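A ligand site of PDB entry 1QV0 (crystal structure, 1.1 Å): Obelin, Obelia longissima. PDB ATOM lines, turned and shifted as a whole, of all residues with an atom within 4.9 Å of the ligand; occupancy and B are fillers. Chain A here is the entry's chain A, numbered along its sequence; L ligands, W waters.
Residues that only touch the ligand: Met 25 (3.3 Å), Leu 29 (3.9 Å), Ile 42 (3.6 Å), Lys 45 (3.9 Å), Ile 50 (3.5 Å), Phe 72 (3.9 Å), Phe 88 (3.2 Å), Ile 111 (3.8 Å), Trp 114 (3.5 Å), Gly 115 (3.3 Å), Phe 119 (3.6 Å), Trp 135 (3.8 Å), Ile 144 (3.3 Å) and Met 171 (3.4 Å).
The nearest printed residue that does not touch the ligand is Val 118 (4.1 Å).
The side-chain hydroxyl (OH) of Tyr 190 lies within hydrogen-bond range of an oxygen (O5) of the ligand (2.4 Å).
A nitrogen (N1) of the ligand sits at hydrogen-bond distance from the side-chain hydroxyl (OH) of Tyr 138.
O3 of the ligand sits at hydrogen-bond distance from ND1 of His 22 (2.7 Å).
A ring nitrogen (NE2) of His 175 sits close to an oxygen (O2) of the ligand (3.2 Å).
The indole nitrogen (NE1) of Trp 179 is in hydrogen-bond range of an oxygen (O2) of the ligand (3.2 Å).
NE1 of Trp 92 lies within hydrogen-bond range of O3 of the ligand (3.3 Å).
Water W2 lies within hydrogen-bond range of O1 of the ligand (2.7 Å), OG1 of Thr 172 (2.7 Å) and O of Ile 111 (2.8 Å).
A ring nitrogen (NE2) of His 175 is in hydrogen-bond range of the side-chain hydroxyl (OH) of Tyr 190 (2.7 Å).
O of Tyr 138 lies within hydrogen-bond range of OG of Ser 142 (2.8 Å).
A ring nitrogen (NE2) of His 22 lies within hydrogen-bond range of the backbone carbonyl oxygen (O) of Trp 179 (3.0 Å).
OG of Ser 142 sits at hydrogen-bond distance from N of Ile 144 (3.1 Å).
O of Lys 45 sits at hydrogen-bond distance from N of Ile 50, at 2.9 Å.
The backbone carbonyl oxygen of Ser 142 sits at hydrogen-bond distance from the side-chain amino group of Lys 45.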
ATOM      1  N   HIS A  22       2.923  35.514  -2.460  1.00  0.00           N
ATOM      2  CA  HIS A  22       2.848  34.091  -2.099  1.00  0.00           C
ATOM      3  C   HIS A  22       2.726  33.856  -0.628  1.00  0.00           C
ATOM      4  O   HIS A  22       2.122  32.835  -0.239  1.00  0.00           O
ATOM      5  CB  HIS A  22       4.058  33.368  -2.712  1.00  0.00           C
ATOM      6  CG  HIS A  22       3.912  33.236  -4.185  1.00  0.00           C
ATOM      7  ND1 HIS A  22       2.969  32.361  -4.706  1.00  0.00           N
ATOM      8  CD2 HIS A  22       4.527  33.894  -5.203  1.00  0.00           C
ATOM      9  CE1 HIS A  22       3.032  32.468  -6.017  1.00  0.00           C
ATOM     10  NE2 HIS A  22       3.962  33.361  -6.344  1.00  0.00           N
ATOM     11  N   MET A  25      -0.871  33.936   0.031  1.00  0.00           N
ATOM     12  CA  MET A  25      -1.524  32.695  -0.417  1.00  0.00           C
ATOM     13  C   MET A  25      -1.195  31.545   0.522  1.00  0.00           C
ATOM     14  O   MET A  25      -2.065  30.747   0.851  1.00  0.00           O
ATOM     15  CB  MET A  25      -1.124  32.376  -1.827  1.00  0.00           C
ATOM     16  CG  MET A  25      -1.681  33.374  -2.838  1.00  0.00           C
ATOM     17  SD  MET A  25      -3.481  33.645  -2.754  1.00  0.00           S
ATOM     18  CE  MET A  25      -4.085  32.018  -3.122  1.00  0.00           C
ATOM     19  N   PHE A  26       0.058  31.445   0.955  1.00  0.00           N
ATOM     20  CA  PHE A  26       0.396  30.375   1.881  1.00  0.00           C
ATOM     21  C   PHE A  26      -0.441  30.497   3.116  1.00  0.00           C
ATOM     22  O   PHE A  26      -0.965  29.508   3.636  1.00  0.00           O
ATOM     23  CB  PHE A  26       1.905  30.494   2.193  1.00  0.00           C
ATOM     24  CG  PHE A  26       2.356  29.366   3.105  1.00  0.00           C
ATOM     25  CD1 PHE A  26       2.905  28.210   2.584  1.00  0.00           C
ATOM     26  CD2 PHE A  26       2.263  29.490   4.497  1.00  0.00           C
ATOM     27  CE1 PHE A  26       3.333  27.190   3.403  1.00  0.00           C
ATOM     28  CE2 PHE A  26       2.618  28.484   5.321  1.00  0.00           C
ATOM     29  CZ  PHE A  26       3.170  27.321   4.785  1.00  0.00           C
ATOM     30  N   PHE A  28      -3.248  31.871   3.547  1.00  0.00           N
ATOM     31  CA  PHE A  28      -4.616  31.521   3.183  1.00  0.00           C
ATOM     32  C   PHE A  28      -4.803  30.018   3.123  1.00  0.00           C
ATOM     33  O   PHE A  28      -5.857  29.519   3.514  1.00  0.00           O
ATOM     34  CB  PHE A  28      -4.917  32.182   1.827  1.00  0.00           C
ATOM     35  CG  PHE A  28      -5.959  31.518   0.930  1.00  0.00           C
ATOM     36  CD1 PHE A  28      -7.334  31.601   1.140  1.00  0.00           C
ATOM     37  CD2 PHE A  28      -5.485  30.804  -0.179  1.00  0.00           C
ATOM     38  CE1 PHE A  28      -8.236  31.011   0.239  1.00  0.00           C
ATOM     39  CE2 PHE A  28      -6.381  30.211  -1.103  1.00  0.00           C
ATOM     40  CZ  PHE A  28      -7.715  30.308  -0.847  1.00  0.00           C
ATOM     41  N   LEU A  29      -3.797  29.261   2.691  1.00  0.00           N
ATOM     42  CA  LEU A  29      -3.903  27.807   2.688  1.00  0.00           C
ATOM     43  C   LEU A  29      -3.643  27.206   4.038  1.00  0.00           C
ATOM     44  O   LEU A  29      -4.129  26.095   4.324  1.00  0.00           O
ATOM     45  CB  LEU A  29      -2.877  27.261   1.672  1.00  0.00           C
ATOM     46  CG  LEU A  29      -3.216  27.621   0.220  1.00  0.00           C
ATOM     47  CD1 LEU A  29      -2.068  27.229  -0.665  1.00  0.00           C
ATOM     48  CD2 LEU A  29      -4.516  26.931  -0.247  1.00  0.00           C
ATOM     49  N   ILE A  42      -4.363  20.662  -0.056  1.00  0.00           N
ATOM     50  CA  ILE A  42      -4.668  21.388  -1.281  1.00  0.00           C
ATOM     51  C   ILE A  42      -5.581  20.603  -2.150  1.00  0.00           C
ATOM     52  O   ILE A  42      -6.507  21.133  -2.752  1.00  0.00           O
ATOM     53  CB  ILE A  42      -3.310  21.755  -1.933  1.00  0.00           C
ATOM     54  CG1 ILE A  42      -2.705  23.017  -1.275  1.00  0.00           C
ATOM     55  CG2 ILE A  42      -3.466  21.947  -3.422  1.00  0.00           C
ATOM     56  CD1 ILE A  42      -2.735  23.145   0.239  1.00  0.00           C
ATOM     57  N   LYS A  45      -9.070  20.604  -0.725  1.00  0.00           N
ATOM     58  CA  LYS A  45      -9.719  21.886  -1.025  1.00  0.00           C
ATOM     59  C   LYS A  45     -10.228  21.838  -2.453  1.00  0.00           C
ATOM     60  O   LYS A  45     -11.345  22.253  -2.757  1.00  0.00           O
ATOM     61  CB  LYS A  45      -8.694  22.992  -0.790  1.00  0.00           C
ATOM     62  CG  LYS A  45      -9.187  24.392  -1.099  1.00  0.00           C
ATOM     63  CD  LYS A  45      -8.109  25.410  -0.869  1.00  0.00           C
ATOM     64  CE  LYS A  45      -8.493  26.834  -1.208  1.00  0.00           C
ATOM     65  NZ  LYS A  45      -9.552  27.271  -0.216  1.00  0.00           N
ATOM     66  N   ALA A  46      -9.384  21.398  -3.394  1.00  0.00           N
ATOM     67  CA  ALA A  46      -9.779  21.353  -4.802  1.00  0.00           C
ATOM     68  C   ALA A  46     -10.988  20.448  -5.030  1.00  0.00           C
ATOM     69  O   ALA A  46     -11.893  20.842  -5.736  1.00  0.00           O
ATOM     70  CB  ALA A  46      -8.593  20.917  -5.638  1.00  0.00           C
ATOM     71  N   ILE A  50     -14.118  22.743  -3.428  1.00  0.00           N
ATOM     72  CA  ILE A  50     -14.384  23.549  -4.607  1.00  0.00           C
ATOM     73  C   ILE A  50     -15.182  22.764  -5.625  1.00  0.00           C
ATOM     74  O   ILE A  50     -16.236  23.234  -6.043  1.00  0.00           O
ATOM     75  CB  ILE A  50     -13.080  24.076  -5.214  1.00  0.00           C
ATOM     76  CG1 ILE A  50     -12.436  25.079  -4.264  1.00  0.00           C
ATOM     77  CG2 ILE A  50     -13.318  24.652  -6.605  1.00  0.00           C
ATOM     78  CD1 ILE A  50     -11.010  25.457  -4.620  1.00  0.00           C
ATOM     79  N   VAL A  68      -4.338  19.995 -10.437  1.00  0.00           N
ATOM     80  CA  VAL A  68      -3.883  20.590  -9.158  1.00  0.00           C
ATOM     81  C   VAL A  68      -2.693  19.845  -8.613  1.00  0.00           C
ATOM     82  O   VAL A  68      -1.740  20.465  -8.145  1.00  0.00           O
ATOM     83  CB  VAL A  68      -5.070  20.642  -8.199  1.00  0.00           C
ATOM     84  CG1 VAL A  68      -4.596  20.949  -6.784  1.00  0.00           C
ATOM     85  CG2 VAL A  68      -6.093  21.674  -8.667  1.00  0.00           C
ATOM     86  N   PHE A  72       0.840  21.790  -8.055  1.00  0.00           N
ATOM     87  CA  PHE A  72       1.507  21.949  -6.783  1.00  0.00           C
ATOM     88  C   PHE A  72       2.682  21.018  -6.587  1.00  0.00           C
ATOM     89  O   PHE A  72       3.620  21.379  -5.872  1.00  0.00           O
ATOM     90  CB  PHE A  72       0.468  21.869  -5.662  1.00  0.00           C
ATOM     91  CG  PHE A  72      -0.394  23.114  -5.616  1.00  0.00           C
ATOM     92  CD1 PHE A  72      -1.628  23.168  -6.199  1.00  0.00           C
ATOM     93  CD2 PHE A  72       0.114  24.252  -4.978  1.00  0.00           C
ATOM     94  CE1 PHE A  72      -2.367  24.341  -6.184  1.00  0.00           C
ATOM     95  CE2 PHE A  72      -0.629  25.420  -4.955  1.00  0.00           C
ATOM     96  CZ  PHE A  72      -1.864  25.470  -5.589  1.00  0.00           C
ATOM     97  N   PHE A  88       8.192  26.375   0.365  1.00  0.00           N
ATOM     98  CA  PHE A  88       7.117  26.602  -0.604  1.00  0.00           C
ATOM     99  C   PHE A  88       7.527  27.635  -1.622  1.00  0.00           C
ATOM    100  O   PHE A  88       7.332  27.440  -2.824  1.00  0.00           O
ATOM    101  CB  PHE A  88       5.910  27.052   0.208  1.00  0.00           C
ATOM    102  CG  PHE A  88       4.650  27.288  -0.572  1.00  0.00           C
ATOM    103  CD1 PHE A  88       3.929  26.215  -1.073  1.00  0.00           C
ATOM    104  CD2 PHE A  88       4.147  28.562  -0.786  1.00  0.00           C
ATOM    105  CE1 PHE A  88       2.719  26.454  -1.713  1.00  0.00           C
ATOM    106  CE2 PHE A  88       2.963  28.813  -1.374  1.00  0.00           C
ATOM    107  CZ  PHE A  88       2.239  27.730  -1.845  1.00  0.00           C
ATOM    108  N   TRP A  92       8.017  27.619  -5.655  1.00  0.00           N
ATOM    109  CA  TRP A  92       7.435  28.506  -6.641  1.00  0.00           C
ATOM    110  C   TRP A  92       8.503  29.092  -7.567  1.00  0.00           C
ATOM    111  O   TRP A  92       8.183  29.313  -8.741  1.00  0.00           O
ATOM    112  CB  TRP A  92       6.688  29.633  -5.933  1.00  0.00           C
ATOM    113  CG  TRP A  92       5.277  29.257  -5.655  1.00  0.00           C
ATOM    114  CD1 TRP A  92       4.734  28.686  -4.549  1.00  0.00           C
ATOM    115  CD2 TRP A  92       4.197  29.429  -6.584  1.00  0.00           C
ATOM    116  NE1 TRP A  92       3.400  28.472  -4.693  1.00  0.00           N
ATOM    117  CE2 TRP A  92       3.037  28.930  -5.944  1.00  0.00           C
ATOM    118  CE3 TRP A  92       4.099  29.946  -7.872  1.00  0.00           C
ATOM    119  CZ2 TRP A  92       1.806  28.935  -6.541  1.00  0.00           C
ATOM    120  CZ3 TRP A  92       2.832  29.953  -8.445  1.00  0.00           C
ATOM    121  CH2 TRP A  92       1.706  29.467  -7.785  1.00  0.00           C
ATOM    122  N   ILE A 111      -0.134  25.983 -15.357  1.00  0.00           N
ATOM    123  CA  ILE A 111      -1.219  26.927 -14.984  1.00  0.00           C
ATOM    124  C   ILE A 111      -2.263  27.002 -16.074  1.00  0.00           C
ATOM    125  O   ILE A 111      -3.446  27.145 -15.772  1.00  0.00           O
ATOM    126  CB  ILE A 111      -0.640  28.299 -14.623  1.00  0.00           C
ATOM    127  CG1 ILE A 111      -1.661  29.242 -13.974  1.00  0.00           C
ATOM    128  CG2 ILE A 111       0.068  28.967 -15.805  1.00  0.00           C
ATOM    129  CD1 ILE A 111      -2.395  28.723 -12.767  1.00  0.00           C
ATOM    130  N   TRP A 114      -4.368  23.804 -15.512  1.00  0.00           N
ATOM    131  CA  TRP A 114      -5.288  23.955 -14.387  1.00  0.00           C
ATOM    132  C   TRP A 114      -6.429  24.859 -14.826  1.00  0.00           C
ATOM    133  O   TRP A 114      -7.601  24.542 -14.570  1.00  0.00           O
ATOM    134  CB  TRP A 114      -4.486  24.521 -13.224  1.00  0.00           C
ATOM    135  CG  TRP A 114      -5.295  24.634 -11.959  1.00  0.00           C
ATOM    136  CD1 TRP A 114      -6.522  24.160 -11.654  1.00  0.00           C
ATOM    137  CD2 TRP A 114      -4.866  25.308 -10.779  1.00  0.00           C
ATOM    138  NE1 TRP A 114      -6.946  24.464 -10.405  1.00  0.00           N
ATOM    139  CE2 TRP A 114      -5.910  25.178  -9.831  1.00  0.00           C
ATOM    140  CE3 TRP A 114      -3.710  25.999 -10.413  1.00  0.00           C
ATOM    141  CZ2 TRP A 114      -5.811  25.734  -8.550  1.00  0.00           C
ATOM    142  CZ3 TRP A 114      -3.598  26.544  -9.156  1.00  0.00           C
ATOM    143  CH2 TRP A 114      -4.673  26.394  -8.243  1.00  0.00           C
ATOM    144  N   GLY A 115      -6.120  25.970 -15.490  1.00  0.00           N
ATOM    145  CA  GLY A 115      -7.159  26.843 -15.992  1.00  0.00           C
ATOM    146  C   GLY A 115      -8.117  26.093 -16.894  1.00  0.00           C
ATOM    147  O   GLY A 115      -9.321  26.279 -16.756  1.00  0.00           O
ATOM    148  N   VAL A 118     -10.563  24.268 -14.665  1.00  0.00           N
ATOM    149  CA  VAL A 118     -11.509  25.147 -13.975  1.00  0.00           C
ATOM    150  C   VAL A 118     -12.509  25.678 -14.953  1.00  0.00           C
ATOM    151  O   VAL A 118     -13.716  25.616 -14.689  1.00  0.00           O
ATOM    152  CB  VAL A 118     -10.748  26.296 -13.334  1.00  0.00           C
ATOM    153  CG1 VAL A 118     -11.733  27.278 -12.710  1.00  0.00           C
ATOM    154  CG2 VAL A 118      -9.775  25.790 -12.269  1.00  0.00           C
ATOM    155  N   PHE A 119     -12.020  26.166 -16.099  1.00  0.00           N
ATOM    156  CA  PHE A 119     -12.993  26.688 -17.048  1.00  0.00           C
ATOM    157  C   PHE A 119     -13.947  25.643 -17.523  1.00  0.00           C
ATOM    158  O   PHE A 119     -15.138  25.944 -17.737  1.00  0.00           O
ATOM    159  CB  PHE A 119     -12.235  27.281 -18.241  1.00  0.00           C
ATOM    160  CG  PHE A 119     -11.750  28.698 -18.046  1.00  0.00           C
ATOM    161  CD1 PHE A 119     -10.719  29.051 -17.217  1.00  0.00           C
ATOM    162  CD2 PHE A 119     -12.363  29.695 -18.778  1.00  0.00           C
ATOM    163  CE1 PHE A 119     -10.269  30.368 -17.090  1.00  0.00           C
ATOM    164  CE2 PHE A 119     -11.916  30.995 -18.650  1.00  0.00           C
ATOM    165  CZ  PHE A 119     -10.885  31.360 -17.814  1.00  0.00           C
ATOM    166  N   TRP A 135     -17.046  33.836 -12.080  1.00  0.00           N
ATOM    167  CA  TRP A 135     -15.821  34.184 -11.361  1.00  0.00           C
ATOM    168  C   TRP A 135     -16.114  34.597  -9.932  1.00  0.00           C
ATOM    169  O   TRP A 135     -15.370  34.281  -9.002  1.00  0.00           O
ATOM    170  CB  TRP A 135     -15.098  35.273 -12.137  1.00  0.00           C
ATOM    171  CG  TRP A 135     -13.766  35.621 -11.535  1.00  0.00           C
ATOM    172  CD1 TRP A 135     -13.391  36.856 -11.085  1.00  0.00           C
ATOM    173  CD2 TRP A 135     -12.657  34.748 -11.368  1.00  0.00           C
ATOM    174  NE1 TRP A 135     -12.107  36.802 -10.603  1.00  0.00           N
ATOM    175  CE2 TRP A 135     -11.658  35.534 -10.778  1.00  0.00           C
ATOM    176  CE3 TRP A 135     -12.420  33.401 -11.629  1.00  0.00           C
ATOM    177  CZ2 TRP A 135     -10.395  35.024 -10.437  1.00  0.00           C
ATOM    178  CZ3 TRP A 135     -11.194  32.873 -11.299  1.00  0.00           C
ATOM    179  CH2 TRP A 135     -10.225  33.701 -10.710  1.00  0.00           C
ATOM    180  N   TYR A 138     -16.498  31.459  -8.014  1.00  0.00           N
ATOM    181  CA  TYR A 138     -15.205  30.863  -7.781  1.00  0.00           C
ATOM    182  C   TYR A 138     -14.465  31.602  -6.665  1.00  0.00           C
ATOM    183  O   TYR A 138     -13.857  30.983  -5.798  1.00  0.00           O
ATOM    184  CB  TYR A 138     -14.337  30.813  -9.086  1.00  0.00           C
ATOM    185  CG  TYR A 138     -13.050  30.137  -8.768  1.00  0.00           C
ATOM    186  CD1 TYR A 138     -13.031  28.737  -8.682  1.00  0.00           C
ATOM    187  CD2 TYR A 138     -11.860  30.813  -8.505  1.00  0.00           C
ATOM    188  CE1 TYR A 138     -11.882  28.050  -8.385  1.00  0.00           C
ATOM    189  CE2 TYR A 138     -10.716  30.112  -8.169  1.00  0.00           C
ATOM    190  CZ  TYR A 138     -10.734  28.736  -8.097  1.00  0.00           C
ATOM    191  OH  TYR A 138      -9.563  28.073  -7.755  1.00  0.00           O
ATOM    192  N   SER A 142     -13.530  29.085  -3.749  1.00  0.00           N
ATOM    193  CA  SER A 142     -12.134  28.821  -3.474  1.00  0.00           C
ATOM    194  C   SER A 142     -11.651  29.676  -2.329  1.00  0.00           C
ATOM    195  O   SER A 142     -10.642  29.330  -1.727  1.00  0.00           O
ATOM    196  CB  SER A 142     -11.297  29.170  -4.725  1.00  0.00           C
ATOM    197  OG  SER A 142     -11.206  30.553  -4.899  1.00  0.00           O
ATOM    198  N   ILE A 144     -10.338  32.541  -2.672  1.00  0.00           N
ATOM    199  CA  ILE A 144      -9.219  33.449  -3.028  1.00  0.00           C
ATOM    200  C   ILE A 144      -9.676  34.890  -3.121  1.00  0.00           C
ATOM    201  O   ILE A 144      -8.878  35.807  -2.906  1.00  0.00           O
ATOM    202  CB  ILE A 144      -8.569  32.980  -4.333  1.00  0.00           C
ATOM    203  CG1 ILE A 144      -7.201  33.643  -4.529  1.00  0.00           C
ATOM    204  CG2 ILE A 144      -9.418  33.195  -5.561  1.00  0.00           C
ATOM    205  CD1 ILE A 144      -6.364  33.026  -5.630  1.00  0.00           C
ATOM    206  N   VAL A 168      -9.677  31.773 -21.103  1.00  0.00           N
ATOM    207  CA  VAL A 168      -8.578  31.110 -20.426  1.00  0.00           C
ATOM    208  C   VAL A 168      -7.214  31.501 -20.979  1.00  0.00           C
ATOM    209  O   VAL A 168      -6.242  31.488 -20.289  1.00  0.00           O
ATOM    210  CB  VAL A 168      -8.787  29.583 -20.472  1.00  0.00           C
ATOM    211  CG1 VAL A 168      -8.597  29.065 -21.914  1.00  0.00           C
ATOM    212  CG2 VAL A 168      -7.801  28.911 -19.530  1.00  0.00           C
ATOM    213  N   MET A 171      -6.589  34.694 -19.063  1.00  0.00           N
ATOM    214  CA  MET A 171      -6.325  34.464 -17.639  1.00  0.00           C
ATOM    215  C   MET A 171      -4.973  33.770 -17.463  1.00  0.00           C
ATOM    216  O   MET A 171      -4.273  34.021 -16.488  1.00  0.00           O
ATOM    217  CB  MET A 171      -7.478  33.653 -17.049  1.00  0.00           C
ATOM    218  CG  MET A 171      -7.409  33.642 -15.492  1.00  0.00           C
ATOM    219  SD  MET A 171      -7.366  35.323 -14.834  1.00  0.00           S
ATOM    220  CE  MET A 171      -8.051  35.130 -13.211  1.00  0.00           C
ATOM    221  N   THR A 172      -4.564  32.963 -18.419  1.00  0.00           N
ATOM    222  CA  THR A 172      -3.274  32.297 -18.322  1.00  0.00           C
ATOM    223  C   THR A 172      -2.162  33.323 -18.424  1.00  0.00           C
ATOM    224  O   THR A 172      -1.236  33.310 -17.620  1.00  0.00           O
ATOM    225  CB  THR A 172      -3.132  31.235 -19.411  1.00  0.00           C
ATOM    226  OG1 THR A 172      -4.114  30.219 -19.183  1.00  0.00           O
ATOM    227  CG2 THR A 172      -1.770  30.579 -19.377  1.00  0.00           C
ATOM    228  N   HIS A 175      -2.064  35.167 -15.228  1.00  0.00           N
ATOM    229  CA  HIS A 175      -1.481  34.350 -14.179  1.00  0.00           C
ATOM    230  C   HIS A 175       0.028  34.228 -14.277  1.00  0.00           C
ATOM    231  O   HIS A 175       0.696  34.182 -13.262  1.00  0.00           O
ATOM    232  CB  HIS A 175      -2.130  32.970 -14.162  1.00  0.00           C
ATOM    233  CG  HIS A 175      -3.393  32.955 -13.400  1.00  0.00           C
ATOM    234  ND1 HIS A 175      -4.376  31.995 -13.563  1.00  0.00           N
ATOM    235  CD2 HIS A 175      -3.810  33.773 -12.405  1.00  0.00           C
ATOM    236  CE1 HIS A 175      -5.333  32.245 -12.673  1.00  0.00           C
ATOM    237  NE2 HIS A 175      -5.036  33.311 -11.961  1.00  0.00           N
ATOM    238  N   TRP A 179       1.483  35.399 -10.855  1.00  0.00           N
ATOM    239  CA  TRP A 179       2.086  34.453  -9.954  1.00  0.00           C
ATOM    240  C   TRP A 179       3.571  34.258 -10.197  1.00  0.00           C
ATOM    241  O   TRP A 179       4.286  33.902  -9.265  1.00  0.00           O
ATOM    242  CB  TRP A 179       1.374  33.106 -10.038  1.00  0.00           C
ATOM    243  CG  TRP A 179      -0.057  33.082  -9.692  1.00  0.00           C
ATOM    244  CD1 TRP A 179      -1.076  32.606 -10.477  1.00  0.00           C
ATOM    245  CD2 TRP A 179      -0.680  33.543  -8.490  1.00  0.00           C
ATOM    246  NE1 TRP A 179      -2.273  32.721  -9.848  1.00  0.00           N
ATOM    247  CE2 TRP A 179      -2.052  33.315  -8.608  1.00  0.00           C
ATOM    248  CE3 TRP A 179      -0.200  34.125  -7.305  1.00  0.00           C
ATOM    249  CZ2 TRP A 179      -2.988  33.638  -7.646  1.00  0.00           C
ATOM    250  CZ3 TRP A 179      -1.092  34.454  -6.312  1.00  0.00           C
ATOM    251  CH2 TRP A 179      -2.476  34.204  -6.506  1.00  0.00           C
ATOM    252  N   TYR A 190      -6.561  40.253  -8.934  1.00  0.00           N
ATOM    253  CA  TYR A 190      -7.562  39.803  -7.980  1.00  0.00           C
ATOM    254  C   TYR A 190      -8.045  40.975  -7.126  1.00  0.00           C
ATOM    255  O   TYR A 190      -8.481  40.858  -6.006  1.00  0.00           O
ATOM    256  CB  TYR A 190      -7.006  38.719  -7.017  1.00  0.00           C
ATOM    257  CG  TYR A 190      -6.769  37.404  -7.741  1.00  0.00           C
ATOM    258  CD1 TYR A 190      -5.641  37.099  -8.478  1.00  0.00           C
ATOM    259  CD2 TYR A 190      -7.739  36.432  -7.665  1.00  0.00           C
ATOM    260  CE1 TYR A 190      -5.491  35.849  -9.114  1.00  0.00           C
ATOM    261  CE2 TYR A 190      -7.613  35.200  -8.289  1.00  0.00           C
ATOM    262  CZ  TYR A 190      -6.487  34.931  -9.018  1.00  0.00           C
ATOM    263  OH  TYR A 190      -6.381  33.692  -9.629  1.00  0.00           O
HETATM  264  N1  LIG L   1      -7.232  29.450  -7.943  1.00  0.00           N
HETATM  265  C1  LIG L   1      -6.977  29.832  -9.272  1.00  0.00           C
HETATM  266  C2  LIG L   1      -5.437  30.216  -9.234  1.00  0.00           C
HETATM  267  N2  LIG L   1      -5.029  29.930  -8.015  1.00  0.00           N
HETATM  268  C3  LIG L   1      -3.688  30.135  -7.478  1.00  0.00           C
HETATM  269  C4  LIG L   1      -3.560  29.763  -6.158  1.00  0.00           C
HETATM  270  N3  LIG L   1      -4.652  29.277  -5.354  1.00  0.00           N
HETATM  271  C5  LIG L   1      -5.833  29.123  -5.900  1.00  0.00           C
HETATM  272  C6  LIG L   1      -6.084  29.470  -7.303  1.00  0.00           C
HETATM  273  C7  LIG L   1      -7.454  28.680 -10.218  1.00  0.00           C
HETATM  274  C8  LIG L   1      -7.392  29.076 -11.670  1.00  0.00           C
HETATM  275  C9  LIG L   1      -8.390  29.938 -12.271  1.00  0.00           C
HETATM  276  C10 LIG L   1      -8.274  30.301 -13.649  1.00  0.00           C
HETATM  277  C11 LIG L   1      -7.101  29.858 -14.385  1.00  0.00           C
HETATM  278  C12 LIG L   1      -6.096  29.053 -13.774  1.00  0.00           C
HETATM  279  C13 LIG L   1      -6.237  28.676 -12.425  1.00  0.00           C
HETATM  280  O1  LIG L   1      -7.021  30.255 -15.638  1.00  0.00           O
HETATM  281  O2  LIG L   1      -4.724  30.661 -10.117  1.00  0.00           O
HETATM  282  C14 LIG L   1      -2.298  29.906  -5.480  1.00  0.00           C
HETATM  283  C15 LIG L   1      -2.008  29.162  -4.295  1.00  0.00           C
HETATM  284  C16 LIG L   1      -0.787  29.382  -3.637  1.00  0.00           C
HETATM  285  C17 LIG L   1       0.138  30.370  -4.105  1.00  0.00           C
HETATM  286  C18 LIG L   1      -0.191  31.179  -5.245  1.00  0.00           C
HETATM  287  C19 LIG L   1      -1.395  30.908  -5.913  1.00  0.00           C
HETATM  288  O3  LIG L   1       1.286  30.605  -3.442  1.00  0.00           O
HETATM  289  C20 LIG L   1      -6.957  28.636  -5.036  1.00  0.00           C
HETATM  290  C21 LIG L   1      -6.784  27.171  -4.822  1.00  0.00           C
HETATM  291  C22 LIG L   1      -7.688  26.249  -5.403  1.00  0.00           C
HETATM  292  C23 LIG L   1      -7.561  24.860  -5.164  1.00  0.00           C
HETATM  293  C24 LIG L   1      -6.506  24.404  -4.365  1.00  0.00           C
HETATM  294  C25 LIG L   1      -5.585  25.329  -3.788  1.00  0.00           C
HETATM  295  C26 LIG L   1      -5.663  26.713  -4.048  1.00  0.00           C
HETATM  296  O4  LIG L   1      -7.743  31.015  -9.609  1.00  0.00           O
HETATM  297  O5  LIG L   1      -7.575  31.911  -8.534  1.00  0.00           O
HETATM  298  O   HOH W   1      -9.513  25.273  -8.049  1.00  0.00           O
HETATM  299  O   HOH W   2      -4.562  29.630 -16.563  1.00  0.00           O
